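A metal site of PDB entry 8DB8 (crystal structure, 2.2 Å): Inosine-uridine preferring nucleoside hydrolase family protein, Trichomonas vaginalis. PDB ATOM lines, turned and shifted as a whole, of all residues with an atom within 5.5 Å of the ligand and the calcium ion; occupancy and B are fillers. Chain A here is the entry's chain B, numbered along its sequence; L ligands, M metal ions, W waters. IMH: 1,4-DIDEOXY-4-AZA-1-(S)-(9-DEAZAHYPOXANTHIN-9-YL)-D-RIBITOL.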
ATOM      1  N   THR A   7      -5.074  11.452  -4.507  1.00  0.00           N
ATOM      2  CA  THR A   7      -6.489  11.324  -4.234  1.00  0.00           C
ATOM      3  C   THR A   7      -7.216  10.667  -5.393  1.00  0.00           C
ATOM      4  O   THR A   7      -6.836  10.810  -6.559  1.00  0.00           O
ATOM      5  CB  THR A   7      -7.124  12.700  -3.960  1.00  0.00           C
ATOM      6  OG1 THR A   7      -8.531  12.531  -3.715  1.00  0.00           O
ATOM      7  CG2 THR A   7      -6.945  13.632  -5.157  1.00  0.00           C
ATOM      8  N   ASP A   8      -8.273   9.917  -5.060  1.00  0.00           N
ATOM      9  CA  ASP A   8      -9.265   9.480  -6.036  1.00  0.00           C
ATOM     10  C   ASP A   8     -10.534  10.301  -5.848  1.00  0.00           C
ATOM     11  O   ASP A   8     -11.643   9.772  -5.702  1.00  0.00           O
ATOM     12  CB  ASP A   8      -9.533   7.996  -5.904  1.00  0.00           C
ATOM     13  CG  ASP A   8     -10.038   7.601  -4.533  1.00  0.00           C
ATOM     14  OD1 ASP A   8      -9.854   8.381  -3.577  1.00  0.00           O
ATOM     15  OD2 ASP A   8     -10.631   6.510  -4.408  1.00  0.00           O
ATOM     16  N   GLY A  10     -13.125  11.491  -4.333  1.00  0.00           N
ATOM     17  CA  GLY A  10     -14.511  11.315  -4.037  1.00  0.00           C
ATOM     18  C   GLY A  10     -15.006  12.396  -3.098  1.00  0.00           C
ATOM     19  O   GLY A  10     -14.399  13.452  -2.941  1.00  0.00           O
ATOM     20  N   ASP A  12     -15.448  12.513   0.337  1.00  0.00           N
ATOM     21  CA  ASP A  12     -14.653  12.835   1.517  1.00  0.00           C
ATOM     22  C   ASP A  12     -13.252  13.316   1.141  1.00  0.00           C
ATOM     23  O   ASP A  12     -12.669  14.123   1.876  1.00  0.00           O
ATOM     24  CB  ASP A  12     -14.596  11.630   2.457  1.00  0.00           C
ATOM     25  CG  ASP A  12     -13.847  10.453   1.875  1.00  0.00           C
ATOM     26  OD1 ASP A  12     -13.931  10.236   0.651  1.00  0.00           O
ATOM     27  OD2 ASP A  12     -13.159   9.751   2.659  1.00  0.00           O
ATOM     28  N   ASP A  13     -12.716  12.860   0.006  1.00  0.00           N
ATOM     29  CA  ASP A  13     -11.461  13.408  -0.500  1.00  0.00           C
ATOM     30  C   ASP A  13     -11.536  14.921  -0.617  1.00  0.00           C
ATOM     31  O   ASP A  13     -10.638  15.651  -0.152  1.00  0.00           O
ATOM     32  CB  ASP A  13     -11.120  12.831  -1.880  1.00  0.00           C
ATOM     33  CG  ASP A  13     -11.039  11.324  -1.909  1.00  0.00           C
ATOM     34  OD1 ASP A  13     -12.094  10.658  -1.871  1.00  0.00           O
ATOM     35  OD2 ASP A  13      -9.904  10.800  -2.008  1.00  0.00           O
ATOM     36  N   ASN A  37     -12.543   5.546  -6.144  1.00  0.00           N
ATOM     37  CA  ASN A  37     -13.947   5.879  -5.963  1.00  0.00           C
ATOM     38  C   ASN A  37     -14.645   6.002  -7.312  1.00  0.00           C
ATOM     39  O   ASN A  37     -15.683   5.374  -7.552  1.00  0.00           O
ATOM     40  CB  ASN A  37     -14.070   7.193  -5.176  1.00  0.00           C
ATOM     41  CG  ASN A  37     -13.767   7.013  -3.701  1.00  0.00           C
ATOM     42  OD1 ASN A  37     -13.952   5.928  -3.132  1.00  0.00           O
ATOM     43  ND2 ASN A  37     -13.298   8.090  -3.062  1.00  0.00           N
ATOM     44  N   ILE A  76     -16.970   2.449  -7.359  1.00  0.00           N
ATOM     45  CA  ILE A  76     -18.114   2.324  -6.460  1.00  0.00           C
ATOM     46  C   ILE A  76     -19.085   3.479  -6.694  1.00  0.00           C
ATOM     47  O   ILE A  76     -19.274   4.319  -5.792  1.00  0.00           O
ATOM     48  CB  ILE A  76     -17.672   2.238  -4.998  1.00  0.00           C
ATOM     49  CG1 ILE A  76     -16.673   3.354  -4.654  1.00  0.00           C
ATOM     50  CG2 ILE A  76     -17.034   0.883  -4.703  1.00  0.00           C
ATOM     51  CD1 ILE A  76     -16.226   3.359  -3.197  1.00  0.00           C
ATOM     52  N   ILE A  79     -21.772   4.620  -4.112  1.00  0.00           N
ATOM     53  CA  ILE A  79     -21.341   5.223  -2.860  1.00  0.00           C
ATOM     54  C   ILE A  79     -21.002   6.691  -3.039  1.00  0.00           C
ATOM     55  O   ILE A  79     -21.514   7.562  -2.315  1.00  0.00           O
ATOM     56  CB  ILE A  79     -20.146   4.456  -2.245  1.00  0.00           C
ATOM     57  CG1 ILE A  79     -20.551   3.020  -1.899  1.00  0.00           C
ATOM     58  CG2 ILE A  79     -19.615   5.177  -1.014  1.00  0.00           C
ATOM     59  CD1 ILE A  79     -19.437   2.204  -1.287  1.00  0.00           C
ATOM     60  N   HIS A  80     -20.144   7.008  -4.001  1.00  0.00           N
ATOM     61  CA  HIS A  80     -19.741   8.380  -4.275  1.00  0.00           C
ATOM     62  C   HIS A  80     -20.437   8.971  -5.499  1.00  0.00           C
ATOM     63  O   HIS A  80     -20.106  10.078  -5.906  1.00  0.00           O
ATOM     64  CB  HIS A  80     -18.224   8.460  -4.454  1.00  0.00           C
ATOM     65  CG  HIS A  80     -17.465   8.307  -3.170  1.00  0.00           C
ATOM     66  ND1 HIS A  80     -16.762   9.342  -2.590  1.00  0.00           N
ATOM     67  CD2 HIS A  80     -17.280   7.238  -2.373  1.00  0.00           C
ATOM     68  CE1 HIS A  80     -16.195   8.917  -1.475  1.00  0.00           C
ATOM     69  NE2 HIS A  80     -16.488   7.640  -1.326  1.00  0.00           N
ATOM     70  N   LEU A 125      -4.726   9.612  -0.127  1.00  0.00           N
ATOM     71  CA  LEU A 125      -6.138   9.460   0.180  1.00  0.00           C
ATOM     72  C   LEU A 125      -6.832   8.442  -0.702  1.00  0.00           C
ATOM     73  O   LEU A 125      -8.053   8.492  -0.864  1.00  0.00           O
ATOM     74  CB  LEU A 125      -6.852  10.807   0.054  1.00  0.00           C
ATOM     75  CG  LEU A 125      -6.370  11.949   0.954  1.00  0.00           C
ATOM     76  CD1 LEU A 125      -7.153  13.220   0.655  1.00  0.00           C
ATOM     77  CD2 LEU A 125      -6.497  11.570   2.413  1.00  0.00           C
ATOM     78  N   ALA A 126      -6.088   7.505  -1.277  1.00  0.00           N
ATOM     79  CA  ALA A 126      -6.595   6.701  -2.384  1.00  0.00           C
ATOM     80  C   ALA A 126      -5.740   5.453  -2.504  1.00  0.00           C
ATOM     81  O   ALA A 126      -4.714   5.324  -1.804  1.00  0.00           O
ATOM     82  CB  ALA A 126      -6.597   7.504  -3.687  1.00  0.00           C
ATOM     83  N   MET A 151      -4.457   7.449   4.359  1.00  0.00           N
ATOM     84  CA  MET A 151      -5.779   6.913   4.673  1.00  0.00           C
ATOM     85  C   MET A 151      -5.876   5.517   4.071  1.00  0.00           C
ATOM     86  O   MET A 151      -5.751   5.345   2.853  1.00  0.00           O
ATOM     87  CB  MET A 151      -6.872   7.827   4.104  1.00  0.00           C
ATOM     88  CG  MET A 151      -8.257   7.737   4.751  1.00  0.00           C
ATOM     89  SD  MET A 151      -8.948   6.091   4.975  1.00  0.00           S
ATOM     90  CE  MET A 151      -9.075   5.545   3.295  1.00  0.00           C
ATOM     91  N   ASN A 160     -14.720  -2.146   4.916  1.00  0.00           N
ATOM     92  CA  ASN A 160     -15.976  -1.691   4.345  1.00  0.00           C
ATOM     93  C   ASN A 160     -16.319  -2.438   3.056  1.00  0.00           C
ATOM     94  O   ASN A 160     -17.349  -3.109   2.984  1.00  0.00           O
ATOM     95  CB  ASN A 160     -15.947  -0.177   4.093  1.00  0.00           C
ATOM     96  CG  ASN A 160     -14.601   0.307   3.577  1.00  0.00           C
ATOM     97  OD1 ASN A 160     -13.806  -0.483   3.053  1.00  0.00           O
ATOM     98  ND2 ASN A 160     -14.338   1.598   3.719  1.00  0.00           N
ATOM     99  N   ILE A 161     -15.452  -2.360   2.050  1.00  0.00           N
ATOM    100  CA  ILE A 161     -15.754  -2.960   0.756  1.00  0.00           C
ATOM    101  C   ILE A 161     -15.795  -4.482   0.858  1.00  0.00           C
ATOM    102  O   ILE A 161     -16.572  -5.140   0.162  1.00  0.00           O
ATOM    103  CB  ILE A 161     -14.743  -2.461  -0.303  1.00  0.00           C
ATOM    104  CG1 ILE A 161     -15.319  -2.648  -1.709  1.00  0.00           C
ATOM    105  CG2 ILE A 161     -13.387  -3.142  -0.159  1.00  0.00           C
ATOM    106  CD1 ILE A 161     -16.407  -1.653  -2.041  1.00  0.00           C
ATOM    107  N   GLU A 166     -10.167  -2.619   3.971  1.00  0.00           N
ATOM    108  CA  GLU A 166     -10.497  -1.246   3.655  1.00  0.00           C
ATOM    109  C   GLU A 166     -10.293  -1.005   2.166  1.00  0.00           C
ATOM    110  O   GLU A 166      -9.450  -1.629   1.522  1.00  0.00           O
ATOM    111  CB  GLU A 166      -9.633  -0.293   4.497  1.00  0.00           C
ATOM    112  CG  GLU A 166      -9.844   1.192   4.211  1.00  0.00           C
ATOM    113  CD  GLU A 166      -9.025   1.668   3.031  1.00  0.00           C
ATOM    114  OE1 GLU A 166      -7.943   1.101   2.787  1.00  0.00           O
ATOM    115  OE2 GLU A 166      -9.491   2.587   2.309  1.00  0.00           O
ATOM    116  N   PHE A 167     -11.083  -0.075   1.613  1.00  0.00           N
ATOM    117  CA  PHE A 167     -11.226   0.040   0.165  1.00  0.00           C
ATOM    118  C   PHE A 167      -9.898   0.345  -0.522  1.00  0.00           C
ATOM    119  O   PHE A 167      -9.511  -0.337  -1.477  1.00  0.00           O
ATOM    120  CB  PHE A 167     -12.263   1.110  -0.174  1.00  0.00           C
ATOM    121  CG  PHE A 167     -12.274   1.491  -1.635  1.00  0.00           C
ATOM    122  CD1 PHE A 167     -12.930   0.689  -2.552  1.00  0.00           C
ATOM    123  CD2 PHE A 167     -11.627   2.617  -2.078  1.00  0.00           C
ATOM    124  CE1 PHE A 167     -12.938   1.016  -3.899  1.00  0.00           C
ATOM    125  CE2 PHE A 167     -11.628   2.955  -3.421  1.00  0.00           C
ATOM    126  CZ  PHE A 167     -12.295   2.158  -4.331  1.00  0.00           C
ATOM    127  N   ASN A 168      -9.202   1.398  -0.076  1.00  0.00           N
ATOM    128  CA  ASN A 168      -8.004   1.846  -0.787  1.00  0.00           C
ATOM    129  C   ASN A 168      -6.950   0.745  -0.857  1.00  0.00           C
ATOM    130  O   ASN A 168      -6.316   0.548  -1.897  1.00  0.00           O
ATOM    131  CB  ASN A 168      -7.424   3.079  -0.098  1.00  0.00           C
ATOM    132  CG  ASN A 168      -8.245   4.324  -0.352  1.00  0.00           C
ATOM    133  OD1 ASN A 168      -9.165   4.315  -1.164  1.00  0.00           O
ATOM    134  ND2 ASN A 168      -7.904   5.400   0.344  1.00  0.00           N
ATOM    135  N   TRP A 193      -9.698   2.809   8.342  1.00  0.00           N
ATOM    136  CA  TRP A 193     -11.156   2.723   8.422  1.00  0.00           C
ATOM    137  C   TRP A 193     -11.602   2.447   9.848  1.00  0.00           C
ATOM    138  O   TRP A 193     -12.733   2.780  10.220  1.00  0.00           O
ATOM    139  CB  TRP A 193     -11.660   1.633   7.477  1.00  0.00           C
ATOM    140  CG  TRP A 193     -13.163   1.541   7.396  1.00  0.00           C
ATOM    141  CD1 TRP A 193     -13.932   0.490   7.806  1.00  0.00           C
ATOM    142  CD2 TRP A 193     -14.067   2.512   6.860  1.00  0.00           C
ATOM    143  NE1 TRP A 193     -15.257   0.750   7.567  1.00  0.00           N
ATOM    144  CE2 TRP A 193     -15.370   1.987   6.989  1.00  0.00           C
ATOM    145  CE3 TRP A 193     -13.905   3.776   6.278  1.00  0.00           C
ATOM    146  CZ2 TRP A 193     -16.505   2.686   6.557  1.00  0.00           C
ATOM    147  CZ3 TRP A 193     -15.034   4.465   5.862  1.00  0.00           C
ATOM    148  CH2 TRP A 193     -16.308   3.921   6.005  1.00  0.00           C
ATOM    149  N   ILE A 227     -23.840  10.226   0.066  1.00  0.00           N
ATOM    150  CA  ILE A 227     -23.083   9.255   0.864  1.00  0.00           C
ATOM    151  C   ILE A 227     -23.594   9.208   2.299  1.00  0.00           C
ATOM    152  O   ILE A 227     -23.483   8.173   2.958  1.00  0.00           O
ATOM    153  CB  ILE A 227     -21.579   9.553   0.792  1.00  0.00           C
ATOM    154  CG1 ILE A 227     -20.773   8.257   0.869  1.00  0.00           C
ATOM    155  CG2 ILE A 227     -21.156  10.504   1.898  1.00  0.00           C
ATOM    156  CD1 ILE A 227     -19.282   8.469   0.759  1.00  0.00           C
ATOM    157  N   PHE A 230     -26.499   6.926   1.969  1.00  0.00           N
ATOM    158  CA  PHE A 230     -26.027   5.561   1.745  1.00  0.00           C
ATOM    159  C   PHE A 230     -25.529   4.927   3.035  1.00  0.00           C
ATOM    160  O   PHE A 230     -25.633   3.697   3.198  1.00  0.00           O
ATOM    161  CB  PHE A 230     -24.913   5.558   0.688  1.00  0.00           C
ATOM    162  CG  PHE A 230     -23.978   4.384   0.798  1.00  0.00           C
ATOM    163  CD1 PHE A 230     -22.759   4.502   1.441  1.00  0.00           C
ATOM    164  CD2 PHE A 230     -24.334   3.149   0.254  1.00  0.00           C
ATOM    165  CE1 PHE A 230     -21.903   3.415   1.548  1.00  0.00           C
ATOM    166  CE2 PHE A 230     -23.480   2.068   0.353  1.00  0.00           C
ATOM    167  CZ  PHE A 230     -22.264   2.202   1.007  1.00  0.00           C
ATOM    168  N   ASP A 231     -25.006   5.717   3.954  1.00  0.00           N
ATOM    169  CA  ASP A 231     -24.453   5.199   5.200  1.00  0.00           C
ATOM    170  C   ASP A 231     -25.493   5.083   6.304  1.00  0.00           C
ATOM    171  O   ASP A 231     -25.170   4.575   7.389  1.00  0.00           O
ATOM    172  CB  ASP A 231     -23.307   6.099   5.676  1.00  0.00           C
ATOM    173  CG  ASP A 231     -21.947   5.461   5.462  1.00  0.00           C
ATOM    174  OD1 ASP A 231     -21.873   4.222   5.347  1.00  0.00           O
ATOM    175  OD2 ASP A 231     -20.951   6.209   5.398  1.00  0.00           O
ATOM    176  N   CYS A 236     -18.629   8.662   8.207  1.00  0.00           N
ATOM    177  CA  CYS A 236     -17.316   8.129   8.535  1.00  0.00           C
ATOM    178  C   CYS A 236     -16.264   8.973   7.819  1.00  0.00           C
ATOM    179  O   CYS A 236     -15.841   8.629   6.709  1.00  0.00           O
ATOM    180  CB  CYS A 236     -17.186   6.656   8.151  1.00  0.00           C
ATOM    181  SG  CYS A 236     -18.666   5.673   8.518  1.00  0.00           S
ATOM    182  N   ALA A 238     -13.407   9.473   6.651  1.00  0.00           N
ATOM    183  CA  ALA A 238     -12.113   8.795   6.547  1.00  0.00           C
ATOM    184  C   ALA A 238     -11.035   9.726   6.014  1.00  0.00           C
ATOM    185  O   ALA A 238     -10.029   9.976   6.679  1.00  0.00           O
ATOM    186  CB  ALA A 238     -12.251   7.560   5.654  1.00  0.00           C
ATOM    187  N   ASP A 239     -11.216  10.246   4.789  1.00  0.00           N
ATOM    188  CA  ASP A 239     -10.193  11.130   4.221  1.00  0.00           C
ATOM    189  C   ASP A 239     -10.059  12.428   5.006  1.00  0.00           C
ATOM    190  O   ASP A 239      -8.920  12.857   5.257  1.00  0.00           O
ATOM    191  CB  ASP A 239     -10.486  11.380   2.737  1.00  0.00           C
ATOM    192  CG  ASP A 239     -10.073  10.216   1.860  1.00  0.00           C
ATOM    193  OD1 ASP A 239      -9.563   9.206   2.371  1.00  0.00           O
ATOM    194  OD2 ASP A 239     -10.276  10.300   0.635  1.00  0.00           O
HETATM  195  O5' IMH L   1     -12.140   3.065   2.609  1.00  0.00           O
HETATM  196  C5' IMH L   1     -12.318   4.454   2.608  1.00  0.00           C
HETATM  197  C4' IMH L   1     -11.878   5.034   1.292  1.00  0.00           C
HETATM  198  N4' IMH L   1     -12.677   4.683   0.293  1.00  0.00           N
HETATM  199  C3' IMH L   1     -11.884   6.708   1.366  1.00  0.00           C
HETATM  200  O3' IMH L   1     -10.624   7.199   0.784  1.00  0.00           O
HETATM  201  C2' IMH L   1     -12.925   7.127   0.758  1.00  0.00           C
HETATM  202  O2' IMH L   1     -12.639   8.073  -0.343  1.00  0.00           O
HETATM  203  C1' IMH L   1     -13.688   5.824   0.176  1.00  0.00           C
HETATM  204  C9  IMH L   1     -14.832   5.547   0.940  1.00  0.00           C
HETATM  205  C8  IMH L   1     -15.528   6.289   1.856  1.00  0.00           C
HETATM  206  N7  IMH L   1     -16.531   5.534   2.315  1.00  0.00           N
HETATM  207  C5  IMH L   1     -16.466   4.300   1.698  1.00  0.00           C
HETATM  208  C6  IMH L   1     -17.240   3.172   1.814  1.00  0.00           C
HETATM  209  O6  IMH L   1     -18.376   2.876   2.588  1.00  0.00           O
HETATM  210  N1  IMH L   1     -16.965   2.098   1.091  1.00  0.00           N
HETATM  211  C2  IMH L   1     -15.903   2.101   0.241  1.00  0.00           C
HETATM  212  N3  IMH L   1     -15.135   3.213   0.130  1.00  0.00           N
HETATM  213  C4  IMH L   1     -15.416   4.308   0.856  1.00  0.00           C
HETATM  214 CA    CA M   1     -10.418   8.622  -1.123  1.00  0.00          CA
HETATM  215  O   HOH W   1     -10.686   6.257  -1.705  1.00  0.00           O
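Water W1 lies within hydrogen-bond range of the side-chain amide oxygen (OD1) of Asn 168 (2.5 Å), the side-chain carboxylate (OD2) of Asp 8 (2.7 Å), a nitrogen (N4') of the ligand (3.2 Å) and the side-chain amide nitrogen (ND2) of Asn 37 (3.5 Å).
The side-chain amide nitrogen (ND2) of Asn 37 sits close to the side-chain carboxylate (OD1) of Asp 13 (3.1 Å). OD2 of Asp 13 sits close to OG1 of Thr 7 (2.8 Å). The side-chain carboxylate (OD2) of Asp 12 is in hydrogen-bond range of the backbone NH (N) of Asp 239, at 2.9 Å. The side-chain carboxylate of Glu 166 lies within hydrogen-bond range of the backbone NH of Asn 168 (2.7 Å). The backbone NH of Ile 76 lies within hydrogen-bond range of the backbone carbonyl oxygen of Asn 37 (3.2 Å). The side-chain amide oxygen of Asn 160 lies within hydrogen-bond range of the backbone NH of Phe 167 (3.1 Å). The side-chain amide nitrogen (ND2) of Asn 168 sits close to the backbone carbonyl oxygen (O) of Met 151 (3.3 Å). N of Ala 126 sits close to ND2 of Asn 168.
Ile 76 touches the ligand. Ile 79 touches the ligand. His 80 touches the ligand. CE of Met 151 touches O3' of the ligand (3.4 Å). Trp 193 touches the ligand (CZ3 to N7, 3.996 Å). CE1 of Phe 230 touches O6 of the ligand, at 3.7 Å. Within 4 Å of the ligand: Asp 12, Asp 13, Asn 37, Ile 76, Ile 79, His 80, Leu 125, Met 151, Asn 160, Glu 166, Phe 167, Asn 168, Trp 193, Phe 230 and Asp 239. The nearest printed residue that does not touch the ligand is Asp 8 (4.3 Å).
An oxygen (O5') of the ligand sits at hydrogen-bond distance from the side-chain carboxylate of Glu 166 (2.7 Å). The side-chain carboxylate (OD1) of Asp 12 lies close to an oxygen (O2') of the ligand, at 2.7 Å. The side-chain amide nitrogen (ND2) of Asn 37 lies close to an oxygen (O2') of the ligand (2.8 Å). ND2 of Asn 160 lies within hydrogen-bond range of O5' of the ligand (2.9 Å). An oxygen (O3') of the ligand lies close to the side-chain amide nitrogen (ND2) of Asn 168, 3.3 Å away. N of Phe 167 sits close to O5' of the ligand (3.5 Å).
ND2 of Asn 37 touches the calcium ion, 3.5 Å away. Of the 24 residues printed, 5 come within 4 Å of the calcium ion. The nearest printed residue that does not touch the calcium ion is Asp 12 (4.3 Å).
The backbone carbonyl oxygen (O) of Leu 125 binds the calcium ion (2.4 Å). O3' of the ligand binds the calcium ion, 2.4 Å away. OD2 of Asp 13 is bound to the calcium ion. O2' of the ligand binds the calcium ion (2.4 Å). OD2 of Asp 239 is bound to the calcium ion. The calcium ion is bound by water W1, 2.5 Å away. The calcium ion is bound by the side-chain carboxylate (OD1) of Asp 8 (2.5 Å). OD1 of Asp 13 binds the calcium ion (2.7 Å).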
